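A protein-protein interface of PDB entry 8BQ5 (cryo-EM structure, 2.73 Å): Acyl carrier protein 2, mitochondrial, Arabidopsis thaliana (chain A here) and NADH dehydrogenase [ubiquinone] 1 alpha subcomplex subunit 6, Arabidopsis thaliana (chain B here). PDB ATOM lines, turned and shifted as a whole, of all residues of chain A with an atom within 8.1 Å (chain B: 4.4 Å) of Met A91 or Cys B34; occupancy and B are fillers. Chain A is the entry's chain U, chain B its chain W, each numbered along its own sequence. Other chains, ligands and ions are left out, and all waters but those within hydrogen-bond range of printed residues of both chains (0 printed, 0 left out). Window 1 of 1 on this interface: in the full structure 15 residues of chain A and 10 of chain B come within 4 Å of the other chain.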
ATOM      1  N   VAL A  57       6.176 -35.469 -19.307  1.00  0.00           N
ATOM      2  CA  VAL A  57       5.950 -34.059 -18.875  1.00  0.00           C
ATOM      3  C   VAL A  57       6.502 -33.126 -19.957  1.00  0.00           C
ATOM      4  O   VAL A  57       5.742 -32.246 -20.424  1.00  0.00           O
ATOM      5  CB  VAL A  57       6.605 -33.778 -17.508  1.00  0.00           C
ATOM      6  CG1 VAL A  57       6.749 -32.288 -17.240  1.00  0.00           C
ATOM      7  CG2 VAL A  57       5.845 -34.445 -16.372  1.00  0.00           C
ATOM      8  N   ASP A  85       9.440 -20.227 -20.800  1.00  0.00           N
ATOM      9  CA  ASP A  85       8.989 -21.621 -21.064  1.00  0.00           C
ATOM     10  C   ASP A  85       9.894 -22.602 -20.310  1.00  0.00           C
ATOM     11  O   ASP A  85       9.372 -23.613 -19.823  1.00  0.00           O
ATOM     12  CB  ASP A  85       8.927 -21.925 -22.563  1.00  0.00           C
ATOM     13  CG  ASP A  85       7.678 -21.379 -23.233  1.00  0.00           C
ATOM     14  OD1 ASP A  85       6.684 -21.145 -22.517  1.00  0.00           O
ATOM     15  OD2 ASP A  85       7.712 -21.183 -24.464  1.00  0.00           O
ATOM     16  N   SER A  86      11.190 -22.298 -20.200  1.00  0.00           N
ATOM     17  CA  SER A  86      12.152 -23.213 -19.528  1.00  0.00           C
ATOM     18  C   SER A  86      11.874 -23.298 -18.024  1.00  0.00           C
ATOM     19  O   SER A  86      11.925 -24.419 -17.484  1.00  0.00           O
ATOM     20  CB  SER A  86      13.580 -22.806 -19.785  1.00  0.00           C
ATOM     21  OG  SER A  86      14.475 -23.823 -19.366  1.00  0.00           O
ATOM     22  N   VAL A  87      11.588 -22.166 -17.376  1.00  0.00           N
ATOM     23  CA  VAL A  87      11.240 -22.205 -15.922  1.00  0.00           C
ATOM     24  C   VAL A  87       9.924 -22.977 -15.754  1.00  0.00           C
ATOM     25  O   VAL A  87       9.796 -23.701 -14.752  1.00  0.00           O
ATOM     26  CB  VAL A  87      11.198 -20.805 -15.273  1.00  0.00           C
ATOM     27  CG1 VAL A  87      12.545 -20.103 -15.348  1.00  0.00           C
ATOM     28  CG2 VAL A  87      10.102 -19.917 -15.831  1.00  0.00           C
ATOM     29  N   GLU A  88       9.012 -22.868 -16.720  1.00  0.00           N
ATOM     30  CA  GLU A  88       7.696 -23.552 -16.621  1.00  0.00           C
ATOM     31  C   GLU A  88       7.926 -25.064 -16.562  1.00  0.00           C
ATOM     32  O   GLU A  88       7.374 -25.693 -15.650  1.00  0.00           O
ATOM     33  CB  GLU A  88       6.819 -23.172 -17.811  1.00  0.00           C
ATOM     34  CG  GLU A  88       5.365 -22.942 -17.448  1.00  0.00           C
ATOM     35  CD  GLU A  88       4.570 -22.182 -18.497  1.00  0.00           C
ATOM     36  OE1 GLU A  88       3.327 -22.186 -18.409  1.00  0.00           O
ATOM     37  OE2 GLU A  88       5.196 -21.583 -19.396  1.00  0.00           O
ATOM     38  N   VAL A  89       8.709 -25.608 -17.497  1.00  0.00           N
ATOM     39  CA  VAL A  89       9.040 -27.063 -17.509  1.00  0.00           C
ATOM     40  C   VAL A  89       9.547 -27.489 -16.129  1.00  0.00           C
ATOM     41  O   VAL A  89       9.080 -28.524 -15.635  1.00  0.00           O
ATOM     42  CB  VAL A  89      10.086 -27.374 -18.595  1.00  0.00           C
ATOM     43  CG1 VAL A  89      10.599 -28.804 -18.506  1.00  0.00           C
ATOM     44  CG2 VAL A  89       9.549 -27.088 -19.988  1.00  0.00           C
ATOM     45  N   VAL A  90      10.469 -26.729 -15.537  1.00  0.00           N
ATOM     46  CA  VAL A  90      11.056 -27.170 -14.278  1.00  0.00           C
ATOM     47  C   VAL A  90       9.999 -27.246 -13.187  1.00  0.00           C
ATOM     48  O   VAL A  90       9.962 -28.205 -12.408  1.00  0.00           O
ATOM     49  CB  VAL A  90      12.226 -26.256 -13.881  1.00  0.00           C
ATOM     50  CG1 VAL A  90      12.836 -26.737 -12.584  1.00  0.00           C
ATOM     51  CG2 VAL A  90      13.271 -26.266 -14.975  1.00  0.00           C
ATOM     52  N   MET A  91       9.114 -26.256 -13.112  1.00  0.00           N
ATOM     53  CA  MET A  91       8.096 -26.357 -12.077  1.00  0.00           C
ATOM     54  C   MET A  91       7.006 -27.360 -12.458  1.00  0.00           C
ATOM     55  O   MET A  91       6.324 -27.882 -11.571  1.00  0.00           O
ATOM     56  CB  MET A  91       7.509 -24.984 -11.762  1.00  0.00           C
ATOM     57  CG  MET A  91       7.358 -24.747 -10.255  1.00  0.00           C
ATOM     58  SD  MET A  91       6.008 -23.688  -9.796  1.00  0.00           S
ATOM     59  CE  MET A  91       4.675 -24.898  -9.818  1.00  0.00           C
ATOM     60  N   ALA A  92       6.893 -27.698 -13.749  1.00  0.00           N
ATOM     61  CA  ALA A  92       5.975 -28.796 -14.140  1.00  0.00           C
ATOM     62  C   ALA A  92       6.566 -30.099 -13.595  1.00  0.00           C
ATOM     63  O   ALA A  92       5.788 -31.030 -13.323  1.00  0.00           O
ATOM     64  CB  ALA A  92       5.784 -28.845 -15.630  1.00  0.00           C
ATOM     65  N   LEU A  93       7.893 -30.172 -13.463  1.00  0.00           N
ATOM     66  CA  LEU A  93       8.510 -31.317 -12.808  1.00  0.00           C
ATOM     67  C   LEU A  93       8.245 -31.295 -11.309  1.00  0.00           C
ATOM     68  O   LEU A  93       8.237 -32.347 -10.662  1.00  0.00           O
ATOM     69  CB  LEU A  93      10.011 -31.321 -13.091  1.00  0.00           C
ATOM     70  CG  LEU A  93      10.378 -31.417 -14.574  1.00  0.00           C
ATOM     71  CD1 LEU A  93      11.883 -31.341 -14.772  1.00  0.00           C
ATOM     72  CD2 LEU A  93       9.814 -32.688 -15.199  1.00  0.00           C
ATOM     73  N   GLU A  94       8.038 -30.105 -10.739  1.00  0.00           N
ATOM     74  CA  GLU A  94       7.731 -30.006  -9.316  1.00  0.00           C
ATOM     75  C   GLU A  94       6.323 -30.499  -9.013  1.00  0.00           C
ATOM     76  O   GLU A  94       6.087 -31.126  -7.974  1.00  0.00           O
ATOM     77  CB  GLU A  94       7.906 -28.568  -8.824  1.00  0.00           C
ATOM     78  CG  GLU A  94       9.347 -28.121  -8.670  1.00  0.00           C
ATOM     79  CD  GLU A  94       9.483 -26.614  -8.564  1.00  0.00           C
ATOM     80  OE1 GLU A  94       8.937 -26.032  -7.601  1.00  0.00           O
ATOM     81  OE2 GLU A  94      10.140 -26.011  -9.435  1.00  0.00           O
ATOM     82  N   GLU A  95       5.387 -30.205  -9.912  1.00  0.00           N
ATOM     83  CA  GLU A  95       3.980 -30.609  -9.687  1.00  0.00           C
ATOM     84  C   GLU A  95       3.872 -32.127  -9.847  1.00  0.00           C
ATOM     85  O   GLU A  95       3.282 -32.766  -8.960  1.00  0.00           O
ATOM     86  CB  GLU A  95       3.066 -29.851 -10.650  1.00  0.00           C
ATOM     87  CG  GLU A  95       1.593 -30.143 -10.449  1.00  0.00           C
ATOM     88  CD  GLU A  95       1.130 -31.443 -11.079  1.00  0.00           C
ATOM     89  OE1 GLU A  95       1.778 -31.891 -12.044  1.00  0.00           O
ATOM     90  OE2 GLU A  95       0.122 -32.001 -10.605  1.00  0.00           O
ATOM     91  N   GLU A  96       4.451 -32.682 -10.910  1.00  0.00           N
ATOM     92  CA  GLU A  96       4.352 -34.110 -11.185  1.00  0.00           C
ATOM     93  C   GLU A  96       4.961 -34.945 -10.068  1.00  0.00           C
ATOM     94  O   GLU A  96       4.398 -35.980  -9.692  1.00  0.00           O
ATOM     95  CB  GLU A  96       5.021 -34.434 -12.522  1.00  0.00           C
ATOM     96  CG  GLU A  96       5.531 -35.866 -12.635  1.00  0.00           C
ATOM     97  CD  GLU A  96       4.567 -36.779 -13.364  1.00  0.00           C
ATOM     98  OE1 GLU A  96       4.604 -38.003 -13.117  1.00  0.00           O
ATOM     99  OE2 GLU A  96       3.769 -36.277 -14.183  1.00  0.00           O
ATOM    100  N   PHE A  97       6.095 -34.518  -9.522  1.00  0.00           N
ATOM    101  CA  PHE A  97       6.784 -35.274  -8.490  1.00  0.00           C
ATOM    102  C   PHE A  97       6.533 -34.744  -7.085  1.00  0.00           C
ATOM    103  O   PHE A  97       7.081 -35.293  -6.124  1.00  0.00           O
ATOM    104  CB  PHE A  97       8.283 -35.305  -8.790  1.00  0.00           C
ATOM    105  CG  PHE A  97       8.618 -36.024 -10.060  1.00  0.00           C
ATOM    106  CD1 PHE A  97       8.724 -37.402 -10.082  1.00  0.00           C
ATOM    107  CD2 PHE A  97       8.803 -35.326 -11.238  1.00  0.00           C
ATOM    108  CE1 PHE A  97       9.023 -38.067 -11.252  1.00  0.00           C
ATOM    109  CE2 PHE A  97       9.103 -35.986 -12.410  1.00  0.00           C
ATOM    110  CZ  PHE A  97       9.213 -37.358 -12.416  1.00  0.00           C
ATOM    111  N   GLY A  98       5.722 -33.699  -6.943  1.00  0.00           N
ATOM    112  CA  GLY A  98       5.263 -33.263  -5.639  1.00  0.00           C
ATOM    113  C   GLY A  98       6.335 -32.826  -4.670  1.00  0.00           C
ATOM    114  O   GLY A  98       6.232 -33.121  -3.479  1.00  0.00           O
ATOM    115  N   PHE A  99       7.364 -32.128  -5.141  1.00  0.00           N
ATOM    116  CA  PHE A  99       8.361 -31.561  -4.246  1.00  0.00           C
ATOM    117  C   PHE A  99       8.963 -30.328  -4.900  1.00  0.00           C
ATOM    118  O   PHE A  99       8.916 -30.162  -6.121  1.00  0.00           O
ATOM    119  CB  PHE A  99       9.432 -32.595  -3.870  1.00  0.00           C
ATOM    120  CG  PHE A  99      10.614 -32.623  -4.794  1.00  0.00           C
ATOM    121  CD1 PHE A  99      11.751 -31.882  -4.519  1.00  0.00           C
ATOM    122  CD2 PHE A  99      10.596 -33.413  -5.929  1.00  0.00           C
ATOM    123  CE1 PHE A  99      12.837 -31.916  -5.367  1.00  0.00           C
ATOM    124  CE2 PHE A  99      11.680 -33.453  -6.779  1.00  0.00           C
ATOM    125  CZ  PHE A  99      12.801 -32.705  -6.498  1.00  0.00           C
ATOM    126  N   GLU A 100       9.528 -29.458  -4.069  1.00  0.00           N
ATOM    127  CA  GLU A 100      10.044 -28.177  -4.528  1.00  0.00           C
ATOM    128  C   GLU A 100      11.540 -28.285  -4.784  1.00  0.00           C
ATOM    129  O   GLU A 100      12.296 -28.733  -3.917  1.00  0.00           O
ATOM    130  CB  GLU A 100       9.762 -27.081  -3.501  1.00  0.00           C
ATOM    131  CG  GLU A 100       8.298 -26.960  -3.105  1.00  0.00           C
ATOM    132  CD  GLU A 100       7.409 -26.584  -4.271  1.00  0.00           C
ATOM    133  OE1 GLU A 100       7.703 -25.575  -4.937  1.00  0.00           O
ATOM    134  OE2 GLU A 100       6.416 -27.297  -4.525  1.00  0.00           O
ATOM    135  N   ILE A 101      11.959 -27.875  -5.971  1.00  0.00           N
ATOM    136  CA  ILE A 101      13.363 -27.903  -6.372  1.00  0.00           C
ATOM    137  C   ILE A 101      14.002 -26.583  -5.957  1.00  0.00           C
ATOM    138  O   ILE A 101      13.518 -25.521  -6.373  1.00  0.00           O
ATOM    139  CB  ILE A 101      13.513 -28.133  -7.885  1.00  0.00           C
ATOM    140  CG1 ILE A 101      12.858 -29.455  -8.284  1.00  0.00           C
ATOM    141  CG2 ILE A 101      14.979 -28.103  -8.283  1.00  0.00           C
ATOM    142  CD1 ILE A 101      13.084 -29.838  -9.725  1.00  0.00           C
ATOM    143  N   ASP A 103      16.095 -23.339  -6.203  1.00  0.00           N
ATOM    144  CA  ASP A 103      16.319 -22.625  -7.495  1.00  0.00           C
ATOM    145  C   ASP A 103      17.672 -22.948  -8.137  1.00  0.00           C
ATOM    146  O   ASP A 103      17.703 -23.140  -9.357  1.00  0.00           O
ATOM    147  CB  ASP A 103      16.173 -21.114  -7.320  1.00  0.00           C
ATOM    148  CG  ASP A 103      14.747 -20.683  -7.011  1.00  0.00           C
ATOM    149  OD1 ASP A 103      13.856 -21.558  -7.007  1.00  0.00           O
ATOM    150  OD2 ASP A 103      14.539 -19.477  -6.773  1.00  0.00           O
ATOM    151  N   ALA A 106      17.145 -25.791  -9.923  1.00  0.00           N
ATOM    152  CA  ALA A 106      16.195 -25.519 -11.026  1.00  0.00           C
ATOM    153  C   ALA A 106      16.947 -24.958 -12.236  1.00  0.00           C
ATOM    154  O   ALA A 106      16.402 -25.048 -13.347  1.00  0.00           O
ATOM    155  CB  ALA A 106      15.140 -24.561 -10.548  1.00  0.00           C
ATOM    156  N   ILE A 109      19.111 -27.597 -14.388  1.00  0.00           N
ATOM    157  CA  ILE A 109      18.210 -28.555 -15.096  1.00  0.00           C
ATOM    158  C   ILE A 109      17.919 -27.907 -16.452  1.00  0.00           C
ATOM    159  O   ILE A 109      16.863 -27.258 -16.615  1.00  0.00           O
ATOM    160  CB  ILE A 109      16.939 -28.871 -14.278  1.00  0.00           C
ATOM    161  CG1 ILE A 109      17.266 -29.655 -13.005  1.00  0.00           C
ATOM    162  CG2 ILE A 109      15.897 -29.592 -15.112  1.00  0.00           C
ATOM    163  CD1 ILE A 109      16.047 -30.057 -12.210  1.00  0.00           C
ATOM    164  N   PHE B  30       6.959 -15.399 -10.808  1.00  0.00           N
ATOM    165  CA  PHE B  30       6.291 -16.521 -11.518  1.00  0.00           C
ATOM    166  C   PHE B  30       6.392 -17.789 -10.664  1.00  0.00           C
ATOM    167  O   PHE B  30       5.389 -18.493 -10.543  1.00  0.00           O
ATOM    168  CB  PHE B  30       6.885 -16.762 -12.907  1.00  0.00           C
ATOM    169  CG  PHE B  30       6.205 -17.870 -13.672  1.00  0.00           C
ATOM    170  CD1 PHE B  30       4.848 -17.809 -13.948  1.00  0.00           C
ATOM    171  CD2 PHE B  30       6.911 -18.986 -14.087  1.00  0.00           C
ATOM    172  CE1 PHE B  30       4.215 -18.830 -14.637  1.00  0.00           C
ATOM    173  CE2 PHE B  30       6.279 -20.006 -14.778  1.00  0.00           C
ATOM    174  CZ  PHE B  30       4.932 -19.927 -15.051  1.00  0.00           C
ATOM    175  N   ARG B  31       7.567 -18.059 -10.091  1.00  0.00           N
ATOM    176  CA  ARG B  31       7.726 -19.231  -9.238  1.00  0.00           C
ATOM    177  C   ARG B  31       6.818 -19.154  -8.018  1.00  0.00           C
ATOM    178  O   ARG B  31       6.140 -20.128  -7.678  1.00  0.00           O
ATOM    179  CB  ARG B  31       9.182 -19.360  -8.799  1.00  0.00           C
ATOM    180  CG  ARG B  31      10.154 -19.630  -9.924  1.00  0.00           C
ATOM    181  CD  ARG B  31      11.250 -20.583  -9.485  1.00  0.00           C
ATOM    182  NE  ARG B  31      12.279 -20.762 -10.504  1.00  0.00           N
ATOM    183  CZ  ARG B  31      13.104 -19.812 -10.927  1.00  0.00           C
ATOM    184  NH1 ARG B  31      13.059 -18.584 -10.435  1.00  0.00           N
ATOM    185  NH2 ARG B  31      14.005 -20.106 -11.860  1.00  0.00           N
ATOM    186  N   ALA B  32       6.794 -18.000  -7.348  1.00  0.00           N
ATOM    187  CA  ALA B  32       6.026 -17.875  -6.113  1.00  0.00           C
ATOM    188  C   ALA B  32       4.528 -17.908  -6.381  1.00  0.00           C
ATOM    189  O   ALA B  32       3.772 -18.546  -5.641  1.00  0.00           O
ATOM    190  CB  ALA B  32       6.411 -16.589  -5.385  1.00  0.00           C
ATOM    191  N   ALA B  33       4.077 -17.214  -7.429  1.00  0.00           N
ATOM    192  CA  ALA B  33       2.652 -17.198  -7.737  1.00  0.00           C
ATOM    193  C   ALA B  33       2.162 -18.573  -8.158  1.00  0.00           C
ATOM    194  O   ALA B  33       1.060 -18.988  -7.782  1.00  0.00           O
ATOM    195  CB  ALA B  33       2.351 -16.169  -8.826  1.00  0.00           C
ATOM    196  N   CYS B  34       2.955 -19.286  -8.968  1.00  0.00           N
ATOM    197  CA  CYS B  34       2.533 -20.605  -9.528  1.00  0.00           C
ATOM    198  C   CYS B  34       2.665 -21.718  -8.489  1.00  0.00           C
ATOM    199  O   CYS B  34       1.902 -22.694  -8.562  1.00  0.00           O
ATOM    200  CB  CYS B  34       3.386 -20.951 -10.742  1.00  0.00           C
ATOM    201  SG  CYS B  34       2.861 -22.435 -11.634  1.00  0.00           S
ATOM    202  N   ARG B  35       3.598 -21.580  -7.556  1.00  0.00           N
ATOM    203  CA  ARG B  35       3.720 -22.571  -6.485  1.00  0.00           C
ATOM    204  C   ARG B  35       2.501 -22.602  -5.570  1.00  0.00           C
ATOM    205  O   ARG B  35       2.295 -23.596  -4.864  1.00  0.00           O
ATOM    206  CB  ARG B  35       4.969 -22.306  -5.638  1.00  0.00           C
ATOM    207  CG  ARG B  35       6.262 -22.866  -6.207  1.00  0.00           C
ATOM    208  CD  ARG B  35       7.427 -22.625  -5.254  1.00  0.00           C
ATOM    209  NE  ARG B  35       8.599 -23.416  -5.611  1.00  0.00           N
ATOM    210  CZ  ARG B  35       9.769 -22.910  -5.975  1.00  0.00           C
ATOM    211  NH1 ARG B  35       9.968 -21.604  -6.034  1.00  0.00           N
ATOM    212  NH2 ARG B  35      10.768 -23.735  -6.276  1.00  0.00           N
ATOM    213  N   SER B  36       1.699 -21.543  -5.560  1.00  0.00           N
ATOM    214  CA  SER B  36       0.544 -21.427  -4.681  1.00  0.00           C
ATOM    215  C   SER B  36      -0.746 -21.935  -5.313  1.00  0.00           C
ATOM    216  O   SER B  36      -1.818 -21.747  -4.729  1.00  0.00           O
ATOM    217  CB  SER B  36       0.360 -19.971  -4.253  1.00  0.00           C
ATOM    218  OG  SER B  36       0.126 -19.148  -5.381  1.00  0.00           O
ATOM    219  N   ILE B  37      -0.661 -22.487  -6.519  1.00  0.00           N
ATOM    220  CA  ILE B  37      -1.867 -23.065  -7.185  1.00  0.00           C
ATOM    221  C   ILE B  37      -2.510 -24.158  -6.304  1.00  0.00           C
ATOM    222  O   ILE B  37      -3.721 -24.066  -6.128  1.00  0.00           O
ATOM    223  CB  ILE B  37      -1.530 -23.516  -8.623  1.00  0.00           C
ATOM    224  CG1 ILE B  37      -1.363 -22.309  -9.546  1.00  0.00           C
ATOM    225  CG2 ILE B  37      -2.562 -24.487  -9.170  1.00  0.00           C
ATOM    226  CD1 ILE B  37      -0.915 -22.675 -10.930  1.00  0.00           C
ATOM    227  N   ARG B  56      -1.755 -22.318 -14.322  1.00  0.00           N
ATOM    228  CA  ARG B  56      -0.310 -22.026 -14.529  1.00  0.00           C
ATOM    229  C   ARG B  56      -0.160 -21.306 -15.865  1.00  0.00           C
ATOM    230  O   ARG B  56       0.516 -20.259 -15.899  1.00  0.00           O
ATOM    231  CB  ARG B  56       0.505 -23.323 -14.497  1.00  0.00           C
ATOM    232  CG  ARG B  56       2.012 -23.167 -14.648  1.00  0.00           C
ATOM    233  CD  ARG B  56       2.765 -24.458 -14.364  1.00  0.00           C
ATOM    234  NE  ARG B  56       2.651 -24.871 -12.971  1.00  0.00           N
ATOM    235  CZ  ARG B  56       1.921 -25.889 -12.527  1.00  0.00           C
ATOM    236  NH1 ARG B  56       1.235 -26.638 -13.373  1.00  0.00           N
ATOM    237  NH2 ARG B  56       1.884 -26.155 -11.235  1.00  0.00           N
ATOM    238  N   ILE B  59      -1.261 -17.605 -15.697  1.00  0.00           N
ATOM    239  CA  ILE B  59      -0.230 -16.676 -15.140  1.00  0.00           C
ATOM    240  C   ILE B  59       0.842 -16.427 -16.209  1.00  0.00           C
ATOM    241  O   ILE B  59       1.197 -15.256 -16.420  1.00  0.00           O
ATOM    242  CB  ILE B  59       0.380 -17.210 -13.827  1.00  0.00           C
ATOM    243  CG1 ILE B  59      -0.694 -17.624 -12.819  1.00  0.00           C
ATOM    244  CG2 ILE B  59       1.343 -16.200 -13.221  1.00  0.00           C
ATOM    245  CD1 ILE B  59      -0.206 -18.604 -11.782  1.00  0.00           C
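O of Ile A101 sits at hydrogen-bond distance from NH2 of Arg B35, 3.3 Å away. OE1 of Glu A94 is in salt-bridge range of NH2 of Arg B35 (3.2 Å). The side-chain carboxylate (OE1) of Glu A100 lies within salt-bridge range of the guanidinium group (NE) of Arg B35. The side-chain carboxylate (OD1) of Asp A103 is in salt-bridge range of the guanidinium group (NE) of Arg B31 (3.9 Å). NH2 of Arg B35 lies within salt-bridge range of OD1 of Asp A103.
The side-chain sulfur (SG) of Cys B34 lies within hydrogen-bond range of the guanidinium group (NE) of Arg B56 (2.8 Å). The backbone carbonyl oxygen (O) of Glu A94 is in hydrogen-bond range of the backbone NH (N) of Phe A99, 3.3 Å away.
Val A87 touches Phe B30. NH2 of Arg B31 touches CG1 of Val A87 (3.8 Å). Phe B30 touches Glu A88. CE of Met A91 touches SG of Cys B34 (3.6 Å). Met A91 touches Arg B35. Arg B56 touches Met A91. Glu A95 touches Arg B56.
Of the printed residues of chain B, Val A87 touches Phe B30 (3.8 Å) and Arg B31 (3.8 Å). Val A90 touches none of the printed residues of chain B. Printed residues of chain A within 4 Å of Arg B31: Val A87 (3.8 Å) and Asp A103 (3.7 Å). Printed residues of chain A within 4 Å of Cys B34: Met A91. Of the printed residues of chain A, Arg B35 touches Met A91 (3.7 Å), Glu A94 (3.2 Å), Glu A100 (2.4 Å), Ile A101 (3.3 Å) and Asp A103 (3.8 Å). The nearest residue of chain B that does not touch Met A91 is Arg B31 (4.1 Å). The nearest residue of chain A that does not touch Cys B34 is Glu A88 (6.4 Å).
Of the 21 printed residues of chain A, 8 touch a printed residue of chain B. Along chain A the printed residues that touch a printed residue of chain B span positions 87 to 103. Of the 10 printed residues of chain B, 5 touch a printed residue of chain A. Among the printed residues, 12 pairs touch across the chains.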
